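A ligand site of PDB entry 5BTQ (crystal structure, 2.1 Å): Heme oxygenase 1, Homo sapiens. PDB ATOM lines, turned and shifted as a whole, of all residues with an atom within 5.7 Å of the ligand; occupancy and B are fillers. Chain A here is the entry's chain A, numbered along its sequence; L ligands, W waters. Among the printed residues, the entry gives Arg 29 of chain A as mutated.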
ATOM      1  N   SER A  18       6.428  -1.251 -26.933  1.00  0.00           N
ATOM      2  CA  SER A  18       6.308   0.131 -26.401  1.00  0.00           C
ATOM      3  C   SER A  18       6.983   1.179 -27.266  1.00  0.00           C
ATOM      4  O   SER A  18       6.472   2.316 -27.413  1.00  0.00           O
ATOM      5  CB  SER A  18       6.843   0.193 -24.974  1.00  0.00           C
ATOM      6  OG  SER A  18       7.588  -0.962 -24.650  1.00  0.00           O
ATOM      7  N   LYS A  22       4.919   4.107 -29.439  1.00  0.00           N
ATOM      8  CA  LYS A  22       5.327   5.508 -29.335  1.00  0.00           C
ATOM      9  C   LYS A  22       5.683   6.134 -30.681  1.00  0.00           C
ATOM     10  O   LYS A  22       5.271   7.254 -30.992  1.00  0.00           O
ATOM     11  CB  LYS A  22       6.509   5.636 -28.372  1.00  0.00           C
ATOM     12  CG  LYS A  22       6.981   7.063 -28.230  1.00  0.00           C
ATOM     13  CD  LYS A  22       7.807   7.251 -26.972  1.00  0.00           C
ATOM     14  CE  LYS A  22       8.208   8.714 -26.842  1.00  0.00           C
ATOM     15  NZ  LYS A  22       8.773   8.999 -25.500  1.00  0.00           N
ATOM     16  N   ARG A  29      -0.793  11.759 -31.912  1.00  0.00           N
ATOM     17  CA  ARG A  29      -0.635  12.363 -30.622  1.00  0.00           C
ATOM     18  C   ARG A  29      -0.466  13.888 -30.720  1.00  0.00           C
ATOM     19  O   ARG A  29      -1.022  14.621 -29.907  1.00  0.00           O
ATOM     20  CB  ARG A  29       0.529  11.744 -29.866  1.00  0.00           C
ATOM     21  CG  ARG A  29       0.662  12.319 -28.472  1.00  0.00           C
ATOM     22  CD  ARG A  29       1.850  11.807 -27.713  1.00  0.00           C
ATOM     23  NE  ARG A  29       2.175  12.730 -26.628  1.00  0.00           N
ATOM     24  CZ  ARG A  29       3.155  12.558 -25.739  1.00  0.00           C
ATOM     25  NH1 ARG A  29       3.934  11.480 -25.795  1.00  0.00           N
ATOM     26  NH2 ARG A  29       3.333  13.468 -24.793  1.00  0.00           N
ATOM     27  N   ALA A  32      -3.772  15.391 -31.428  1.00  0.00           N
ATOM     28  CA  ALA A  32      -4.583  15.448 -30.220  1.00  0.00           C
ATOM     29  C   ALA A  32      -4.225  16.681 -29.381  1.00  0.00           C
ATOM     30  O   ALA A  32      -5.108  17.419 -28.950  1.00  0.00           O
ATOM     31  CB  ALA A  32      -4.451  14.157 -29.393  1.00  0.00           C
ATOM     32  N   GLU A  33      -2.937  16.916 -29.196  1.00  0.00           N
ATOM     33  CA  GLU A  33      -2.445  18.124 -28.519  1.00  0.00           C
ATOM     34  C   GLU A  33      -2.830  19.437 -29.222  1.00  0.00           C
ATOM     35  O   GLU A  33      -2.946  20.486 -28.573  1.00  0.00           O
ATOM     36  CB  GLU A  33      -0.924  18.073 -28.422  1.00  0.00           C
ATOM     37  CG  GLU A  33      -0.395  16.966 -27.512  1.00  0.00           C
ATOM     38  CD  GLU A  33       1.105  16.746 -27.686  1.00  0.00           C
ATOM     39  OE1 GLU A  33       1.729  17.465 -28.484  1.00  0.00           O
ATOM     40  OE2 GLU A  33       1.653  15.839 -27.045  1.00  0.00           O
ATOM     41  N   MET A  38      -8.010  21.154 -26.420  1.00  0.00           N
ATOM     42  CA  MET A  38      -6.762  20.875 -25.679  1.00  0.00           C
ATOM     43  C   MET A  38      -5.741  21.999 -25.705  1.00  0.00           C
ATOM     44  O   MET A  38      -5.118  22.281 -24.676  1.00  0.00           O
ATOM     45  CB  MET A  38      -6.046  19.613 -26.207  1.00  0.00           C
ATOM     46  CG  MET A  38      -6.370  18.347 -25.475  1.00  0.00           C
ATOM     47  SD  MET A  38      -5.821  18.445 -23.723  1.00  0.00           S
ATOM     48  CE  MET A  38      -7.435  18.332 -22.980  1.00  0.00           C
ATOM     49  N   GLN A  42      -4.484  23.665 -22.398  1.00  0.00           N
ATOM     50  CA  GLN A  42      -3.024  23.765 -22.100  1.00  0.00           C
ATOM     51  C   GLN A  42      -2.580  25.171 -21.783  1.00  0.00           C
ATOM     52  O   GLN A  42      -1.686  25.359 -20.960  1.00  0.00           O
ATOM     53  CB  GLN A  42      -2.157  23.200 -23.239  1.00  0.00           C
ATOM     54  CG  GLN A  42      -1.884  21.696 -23.087  1.00  0.00           C
ATOM     55  CD  GLN A  42      -1.710  20.925 -24.398  1.00  0.00           C
ATOM     56  OE1 GLN A  42      -1.257  21.465 -25.418  1.00  0.00           O
ATOM     57  NE2 GLN A  42      -2.060  19.639 -24.365  1.00  0.00           N
ATOM     58  N   TYR A 138      -2.888   1.327 -22.664  1.00  0.00           N
ATOM     59  CA  TYR A 138      -1.705   2.164 -22.854  1.00  0.00           C
ATOM     60  C   TYR A 138      -1.992   3.654 -23.105  1.00  0.00           C
ATOM     61  O   TYR A 138      -1.444   4.553 -22.466  1.00  0.00           O
ATOM     62  CB  TYR A 138      -0.892   1.572 -24.036  1.00  0.00           C
ATOM     63  CG  TYR A 138       0.100   2.510 -24.693  1.00  0.00           C
ATOM     64  CD1 TYR A 138       1.368   2.666 -24.183  1.00  0.00           C
ATOM     65  CD2 TYR A 138      -0.250   3.216 -25.819  1.00  0.00           C
ATOM     66  CE1 TYR A 138       2.289   3.516 -24.791  1.00  0.00           C
ATOM     67  CE2 TYR A 138       0.657   4.090 -26.438  1.00  0.00           C
ATOM     68  CZ  TYR A 138       1.934   4.223 -25.926  1.00  0.00           C
ATOM     69  OH  TYR A 138       2.817   5.092 -26.543  1.00  0.00           O
ATOM     70  N   THR A 139      -2.840   3.912 -24.079  1.00  0.00           N
ATOM     71  CA  THR A 139      -3.193   5.258 -24.467  1.00  0.00           C
ATOM     72  C   THR A 139      -3.788   6.078 -23.279  1.00  0.00           C
ATOM     73  O   THR A 139      -3.385   7.217 -22.959  1.00  0.00           O
ATOM     74  CB  THR A 139      -4.238   5.177 -25.594  1.00  0.00           C
ATOM     75  OG1 THR A 139      -3.701   4.440 -26.711  1.00  0.00           O
ATOM     76  CG2 THR A 139      -4.640   6.537 -26.068  1.00  0.00           C
ATOM     77  N   ARG A 140      -4.778   5.489 -22.658  1.00  0.00           N
ATOM     78  CA  ARG A 140      -5.510   6.140 -21.618  1.00  0.00           C
ATOM     79  C   ARG A 140      -4.672   6.264 -20.377  1.00  0.00           C
ATOM     80  O   ARG A 140      -4.430   7.372 -19.901  1.00  0.00           O
ATOM     81  CB  ARG A 140      -6.785   5.360 -21.284  1.00  0.00           C
ATOM     82  CG  ARG A 140      -7.971   5.852 -22.072  1.00  0.00           C
ATOM     83  CD  ARG A 140      -8.708   6.946 -21.327  1.00  0.00           C
ATOM     84  NE  ARG A 140      -8.031   8.215 -21.224  1.00  0.00           N
ATOM     85  CZ  ARG A 140      -8.091   9.195 -22.122  1.00  0.00           C
ATOM     86  NH1 ARG A 140      -8.812   9.061 -23.245  1.00  0.00           N
ATOM     87  NH2 ARG A 140      -7.491  10.353 -21.877  1.00  0.00           N
ATOM     88  N   LEU A 142      -1.368   5.638 -19.499  1.00  0.00           N
ATOM     89  CA  LEU A 142      -0.096   6.338 -19.576  1.00  0.00           C
ATOM     90  C   LEU A 142      -0.194   7.820 -19.961  1.00  0.00           C
ATOM     91  O   LEU A 142       0.540   8.681 -19.434  1.00  0.00           O
ATOM     92  CB  LEU A 142       0.875   5.566 -20.494  1.00  0.00           C
ATOM     93  CG  LEU A 142       1.830   4.606 -19.792  1.00  0.00           C
ATOM     94  CD1 LEU A 142       1.158   3.735 -18.748  1.00  0.00           C
ATOM     95  CD2 LEU A 142       2.567   3.748 -20.812  1.00  0.00           C
ATOM     96  N   GLY A 143      -1.100   8.131 -20.892  1.00  0.00           N
ATOM     97  CA  GLY A 143      -1.428   9.509 -21.173  1.00  0.00           C
ATOM     98  C   GLY A 143      -1.917  10.251 -19.919  1.00  0.00           C
ATOM     99  O   GLY A 143      -1.411  11.315 -19.601  1.00  0.00           O
ATOM    100  N   ASP A 144      -2.889   9.696 -19.221  1.00  0.00           N
ATOM    101  CA  ASP A 144      -3.486  10.374 -18.067  1.00  0.00           C
ATOM    102  C   ASP A 144      -2.517  10.450 -16.886  1.00  0.00           C
ATOM    103  O   ASP A 144      -2.366  11.480 -16.242  1.00  0.00           O
ATOM    104  CB  ASP A 144      -4.784   9.699 -17.668  1.00  0.00           C
ATOM    105  CG  ASP A 144      -5.886   9.895 -18.727  1.00  0.00           C
ATOM    106  OD1 ASP A 144      -5.767  10.850 -19.498  1.00  0.00           O
ATOM    107  OD2 ASP A 144      -6.844   9.109 -18.809  1.00  0.00           O
ATOM    108  N   SER A 146       0.756  10.539 -17.141  1.00  0.00           N
ATOM    109  CA  SER A 146       1.859  11.429 -17.462  1.00  0.00           C
ATOM    110  C   SER A 146       1.494  12.915 -17.389  1.00  0.00           C
ATOM    111  O   SER A 146       2.255  13.698 -16.869  1.00  0.00           O
ATOM    112  CB  SER A 146       2.411  11.099 -18.847  1.00  0.00           C
ATOM    113  OG  SER A 146       2.972   9.833 -18.867  1.00  0.00           O
ATOM    114  N   GLY A 147       0.338  13.288 -17.911  1.00  0.00           N
ATOM    115  CA  GLY A 147      -0.047  14.691 -17.981  1.00  0.00           C
ATOM    116  C   GLY A 147      -0.842  15.218 -16.808  1.00  0.00           C
ATOM    117  O   GLY A 147      -1.164  16.398 -16.776  1.00  0.00           O
ATOM    118  N   VAL A 150       0.617  18.200 -14.528  1.00  0.00           N
ATOM    119  CA  VAL A 150       0.599  19.443 -15.289  1.00  0.00           C
ATOM    120  C   VAL A 150      -0.815  20.006 -15.479  1.00  0.00           C
ATOM    121  O   VAL A 150      -1.065  21.183 -15.268  1.00  0.00           O
ATOM    122  CB  VAL A 150       1.276  19.237 -16.666  1.00  0.00           C
ATOM    123  CG1 VAL A 150       1.073  20.445 -17.583  1.00  0.00           C
ATOM    124  CG2 VAL A 150       2.754  18.957 -16.466  1.00  0.00           C
ATOM    125  N   LEU A 151      -1.735  19.163 -15.907  1.00  0.00           N
ATOM    126  CA  LEU A 151      -3.106  19.594 -16.121  1.00  0.00           C
ATOM    127  C   LEU A 151      -3.822  19.945 -14.836  1.00  0.00           C
ATOM    128  O   LEU A 151      -4.694  20.779 -14.850  1.00  0.00           O
ATOM    129  CB  LEU A 151      -3.897  18.516 -16.825  1.00  0.00           C
ATOM    130  CG  LEU A 151      -3.370  18.222 -18.225  1.00  0.00           C
ATOM    131  CD1 LEU A 151      -3.873  16.865 -18.675  1.00  0.00           C
ATOM    132  CD2 LEU A 151      -3.769  19.333 -19.197  1.00  0.00           C
ATOM    133  N   LYS A 183       5.850   3.637 -15.096  1.00  0.00           N
ATOM    134  CA  LYS A 183       5.830   3.572 -16.574  1.00  0.00           C
ATOM    135  C   LYS A 183       6.881   2.606 -17.140  1.00  0.00           C
ATOM    136  O   LYS A 183       6.625   1.921 -18.132  1.00  0.00           O
ATOM    137  CB  LYS A 183       5.937   4.946 -17.211  1.00  0.00           C
ATOM    138  CG  LYS A 183       4.624   5.702 -17.124  1.00  0.00           C
ATOM    139  CD  LYS A 183       4.640   7.017 -17.834  1.00  0.00           C
ATOM    140  CE  LYS A 183       5.551   8.007 -17.155  1.00  0.00           C
ATOM    141  NZ  LYS A 183       5.617   9.185 -18.069  1.00  0.00           N
ATOM    142  N   ARG A 187       5.883  -0.689 -19.317  1.00  0.00           N
ATOM    143  CA  ARG A 187       6.483  -0.910 -20.642  1.00  0.00           C
ATOM    144  C   ARG A 187       7.094  -2.317 -20.726  1.00  0.00           C
ATOM    145  O   ARG A 187       6.881  -3.076 -21.662  1.00  0.00           O
ATOM    146  CB  ARG A 187       7.571   0.135 -20.882  1.00  0.00           C
ATOM    147  CG  ARG A 187       7.063   1.458 -21.361  1.00  0.00           C
ATOM    148  CD  ARG A 187       8.235   2.356 -21.767  1.00  0.00           C
ATOM    149  NE  ARG A 187       7.790   3.727 -21.691  1.00  0.00           N
ATOM    150  CZ  ARG A 187       8.029   4.559 -20.676  1.00  0.00           C
ATOM    151  NH1 ARG A 187       8.795   4.204 -19.649  1.00  0.00           N
ATOM    152  NH2 ARG A 187       7.496   5.769 -20.728  1.00  0.00           N
ATOM    153  N   ALA A 210      -7.333   4.844 -30.968  1.00  0.00           N
ATOM    154  CA  ALA A 210      -7.612   5.454 -29.658  1.00  0.00           C
ATOM    155  C   ALA A 210      -7.356   6.956 -29.683  1.00  0.00           C
ATOM    156  O   ALA A 210      -8.177   7.740 -29.186  1.00  0.00           O
ATOM    157  CB  ALA A 210      -6.755   4.821 -28.601  1.00  0.00           C
ATOM    158  N   PHE A 211      -6.220   7.376 -30.241  1.00  0.00           N
ATOM    159  CA  PHE A 211      -5.962   8.800 -30.373  1.00  0.00           C
ATOM    160  C   PHE A 211      -7.029   9.503 -31.193  1.00  0.00           C
ATOM    161  O   PHE A 211      -7.476  10.586 -30.826  1.00  0.00           O
ATOM    162  CB  PHE A 211      -4.574   9.071 -30.937  1.00  0.00           C
ATOM    163  CG  PHE A 211      -3.483   8.890 -29.939  1.00  0.00           C
ATOM    164  CD1 PHE A 211      -3.160   9.933 -29.054  1.00  0.00           C
ATOM    165  CD2 PHE A 211      -2.793   7.704 -29.833  1.00  0.00           C
ATOM    166  CE1 PHE A 211      -2.140   9.781 -28.127  1.00  0.00           C
ATOM    167  CE2 PHE A 211      -1.802   7.547 -28.891  1.00  0.00           C
ATOM    168  CZ  PHE A 211      -1.457   8.577 -28.043  1.00  0.00           C
ATOM    169  N   ASN A 214     -10.121  10.164 -29.310  1.00  0.00           N
ATOM    170  CA  ASN A 214      -9.896  11.355 -28.460  1.00  0.00           C
ATOM    171  C   ASN A 214      -9.985  12.675 -29.226  1.00  0.00           C
ATOM    172  O   ASN A 214     -10.561  13.649 -28.722  1.00  0.00           O
ATOM    173  CB  ASN A 214      -8.554  11.281 -27.751  1.00  0.00           C
ATOM    174  CG  ASN A 214      -8.598  10.384 -26.525  1.00  0.00           C
ATOM    175  OD1 ASN A 214      -9.079  10.793 -25.459  1.00  0.00           O
ATOM    176  ND2 ASN A 214      -8.164   9.132 -26.679  1.00  0.00           N
ATOM    177  N   PHE A 218     -12.658  15.709 -28.586  1.00  0.00           N
ATOM    178  CA  PHE A 218     -12.312  17.100 -28.366  1.00  0.00           C
ATOM    179  C   PHE A 218     -12.955  18.021 -29.382  1.00  0.00           C
ATOM    180  O   PHE A 218     -13.381  19.120 -29.025  1.00  0.00           O
ATOM    181  CB  PHE A 218     -10.806  17.328 -28.505  1.00  0.00           C
ATOM    182  CG  PHE A 218      -9.952  16.636 -27.491  1.00  0.00           C
ATOM    183  CD1 PHE A 218     -10.395  16.452 -26.184  1.00  0.00           C
ATOM    184  CD2 PHE A 218      -8.661  16.233 -27.832  1.00  0.00           C
ATOM    185  CE1 PHE A 218      -9.563  15.830 -25.251  1.00  0.00           C
ATOM    186  CE2 PHE A 218      -7.810  15.637 -26.894  1.00  0.00           C
ATOM    187  CZ  PHE A 218      -8.267  15.436 -25.605  1.00  0.00           C
HETATM  188  C1  LIG L   1       3.139  10.598 -22.271  1.00  0.00           C
HETATM  189  N1  LIG L   1       2.019  12.768 -21.931  1.00  0.00           N
HETATM  190  C2  LIG L   1       3.141  12.017 -21.826  1.00  0.00           C
HETATM  191  C3  LIG L   1       4.241  12.726 -21.093  1.00  0.00           C
HETATM  192  C4  LIG L   1       3.675  14.097 -20.843  1.00  0.00           C
HETATM  193  C5  LIG L   1       2.299  13.976 -21.367  1.00  0.00           C
HETATM  194  C6  LIG L   1       4.304  15.284 -20.167  1.00  0.00           C
HETATM  195  C7  LIG L   1       5.606  12.158 -20.747  1.00  0.00           C
HETATM  196  C8  LIG L   1       6.698  12.853 -21.549  1.00  0.00           C
HETATM  197  C9  LIG L   1       6.362  12.953 -23.016  1.00  0.00           C
HETATM  198  O1  LIG L   1       6.264  14.083 -23.576  1.00  0.00           O
HETATM  199  O2  LIG L   1       6.217  11.869 -23.614  1.00  0.00           O
HETATM  200  C10 LIG L   1       1.267  15.063 -21.398  1.00  0.00           C
HETATM  201  N2  LIG L   1      -0.749  13.601 -21.684  1.00  0.00           N
HETATM  202  C11 LIG L   1      -0.195  14.834 -21.518  1.00  0.00           C
HETATM  203  C12 LIG L   1      -1.165  15.967 -21.541  1.00  0.00           C
HETATM  204  C13 LIG L   1      -2.445  15.259 -21.729  1.00  0.00           C
HETATM  205  C14 LIG L   1      -2.070  13.802 -21.814  1.00  0.00           C
HETATM  206  C15 LIG L   1      -0.882  17.435 -21.354  1.00  0.00           C
HETATM  207  O3  LIG L   1      -2.885  12.823 -21.987  1.00  0.00           O
HETATM  208  C16 LIG L   1      -3.775  15.893 -21.863  1.00  0.00           C
HETATM  209  C17 LIG L   1      -4.834  15.214 -22.265  1.00  0.00           C
HETATM  210  N3  LIG L   1      -0.912  12.647 -24.604  1.00  0.00           N
HETATM  211  C18 LIG L   1      -1.748  13.640 -24.984  1.00  0.00           C
HETATM  212  C19 LIG L   1      -3.131  13.271 -25.417  1.00  0.00           C
HETATM  213  C20 LIG L   1      -3.026  11.795 -25.257  1.00  0.00           C
HETATM  214  C21 LIG L   1      -1.650  11.537 -24.761  1.00  0.00           C
HETATM  215  C22 LIG L   1      -4.270  14.152 -25.887  1.00  0.00           C
HETATM  216  O4  LIG L   1      -1.410  14.876 -24.960  1.00  0.00           O
HETATM  217  C23 LIG L   1      -4.022  10.726 -25.481  1.00  0.00           C
HETATM  218  C24 LIG L   1      -5.273  10.978 -25.747  1.00  0.00           C
HETATM  219  C25 LIG L   1      -1.220  10.166 -24.433  1.00  0.00           C
HETATM  220  N4  LIG L   1       0.887  10.685 -23.329  1.00  0.00           N
HETATM  221  C26 LIG L   1       0.106   9.766 -23.954  1.00  0.00           C
HETATM  222  C27 LIG L   1       0.643   8.396 -24.037  1.00  0.00           C
HETATM  223  C28 LIG L   1       1.972   8.533 -23.401  1.00  0.00           C
HETATM  224  C29 LIG L   1       2.010   9.967 -22.998  1.00  0.00           C
HETATM  225  C30 LIG L   1       0.034   7.182 -24.670  1.00  0.00           C
HETATM  226  C31 LIG L   1       3.055   7.481 -23.219  1.00  0.00           C
HETATM  227  C32 LIG L   1       4.099   7.664 -24.300  1.00  0.00           C
HETATM  228  C33 LIG L   1       5.158   6.607 -24.116  1.00  0.00           C
HETATM  229  O5  LIG L   1       6.028   6.881 -23.265  1.00  0.00           O
HETATM  230  O6  LIG L   1       5.103   5.547 -24.809  1.00  0.00           O
HETATM  231  O   HOH W   1      -5.025  13.348 -19.449  1.00  0.00           O
HETATM  232  O   HOH W   2       0.898  15.462 -24.427  1.00  0.00           O
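The guanidinium group (NH1) of Arg 140 is in hydrogen-bond range of the side-chain amide oxygen (OD1) of Asn 214 (2.8 Å).
OG of Ser 146 sits at hydrogen-bond distance from O of Leu 142, at 2.8 Å.
The side-chain amino group of Lys 183 is in hydrogen-bond range of the side-chain hydroxyl of Ser 146 (2.8 Å).
The side-chain carboxylate (OE2) of Glu 33 is in salt-bridge range of the guanidinium group (NE) of Arg 29, 3.2 Å away.
The backbone carbonyl oxygen (O) of Lys 183 sits close to the guanidinium group (NH1) of Arg 187.
The backbone carbonyl oxygen (O) of Ala 210 is in hydrogen-bond range of the side-chain amide nitrogen (ND2) of Asn 214.
Water W2 lies within hydrogen-bond range of an oxygen (O4) of the ligand (2.4 Å), the side-chain carboxylate of Glu 33 (2.8 Å) and the guanidinium group of Arg 29 (3.2 Å).
Water W1 lies within hydrogen-bond range of OD1 of Asp 144 (2.6 Å) and O3 of the ligand (3.4 Å).
O2 of the ligand is in salt-bridge range of NH1 of Arg 29 (3.2 Å).
O of Gly 143 sits at hydrogen-bond distance from N2 of the ligand, 3.2 Å away.
An oxygen (O5) of the ligand lies within salt-bridge range of the guanidinium group (NH2) of Arg 187, at 3.1 Å.
An oxygen (O6) of the ligand sits at hydrogen-bond distance from the side-chain hydroxyl (OH) of Tyr 138 (2.9 Å).
Residues that only touch the ligand: Ser 146, Leu 151, Phe 211, Glu 33, Asn 214, Ala 32, Gly 147, Met 38, Thr 139, Lys 22, Gln 42, Phe 218 and Leu 142.
Hydrophobic or aromatic side chains within 4 Å of the ligand: Ala 32, Met 38, Tyr 138, Leu 142, Leu 151, Phe 211 and Phe 218.
Of the 23 residues printed, 17 come within 4 Å of the ligand.
The nearest printed residue that does not touch the ligand is Lys 183 (4.001 Å).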
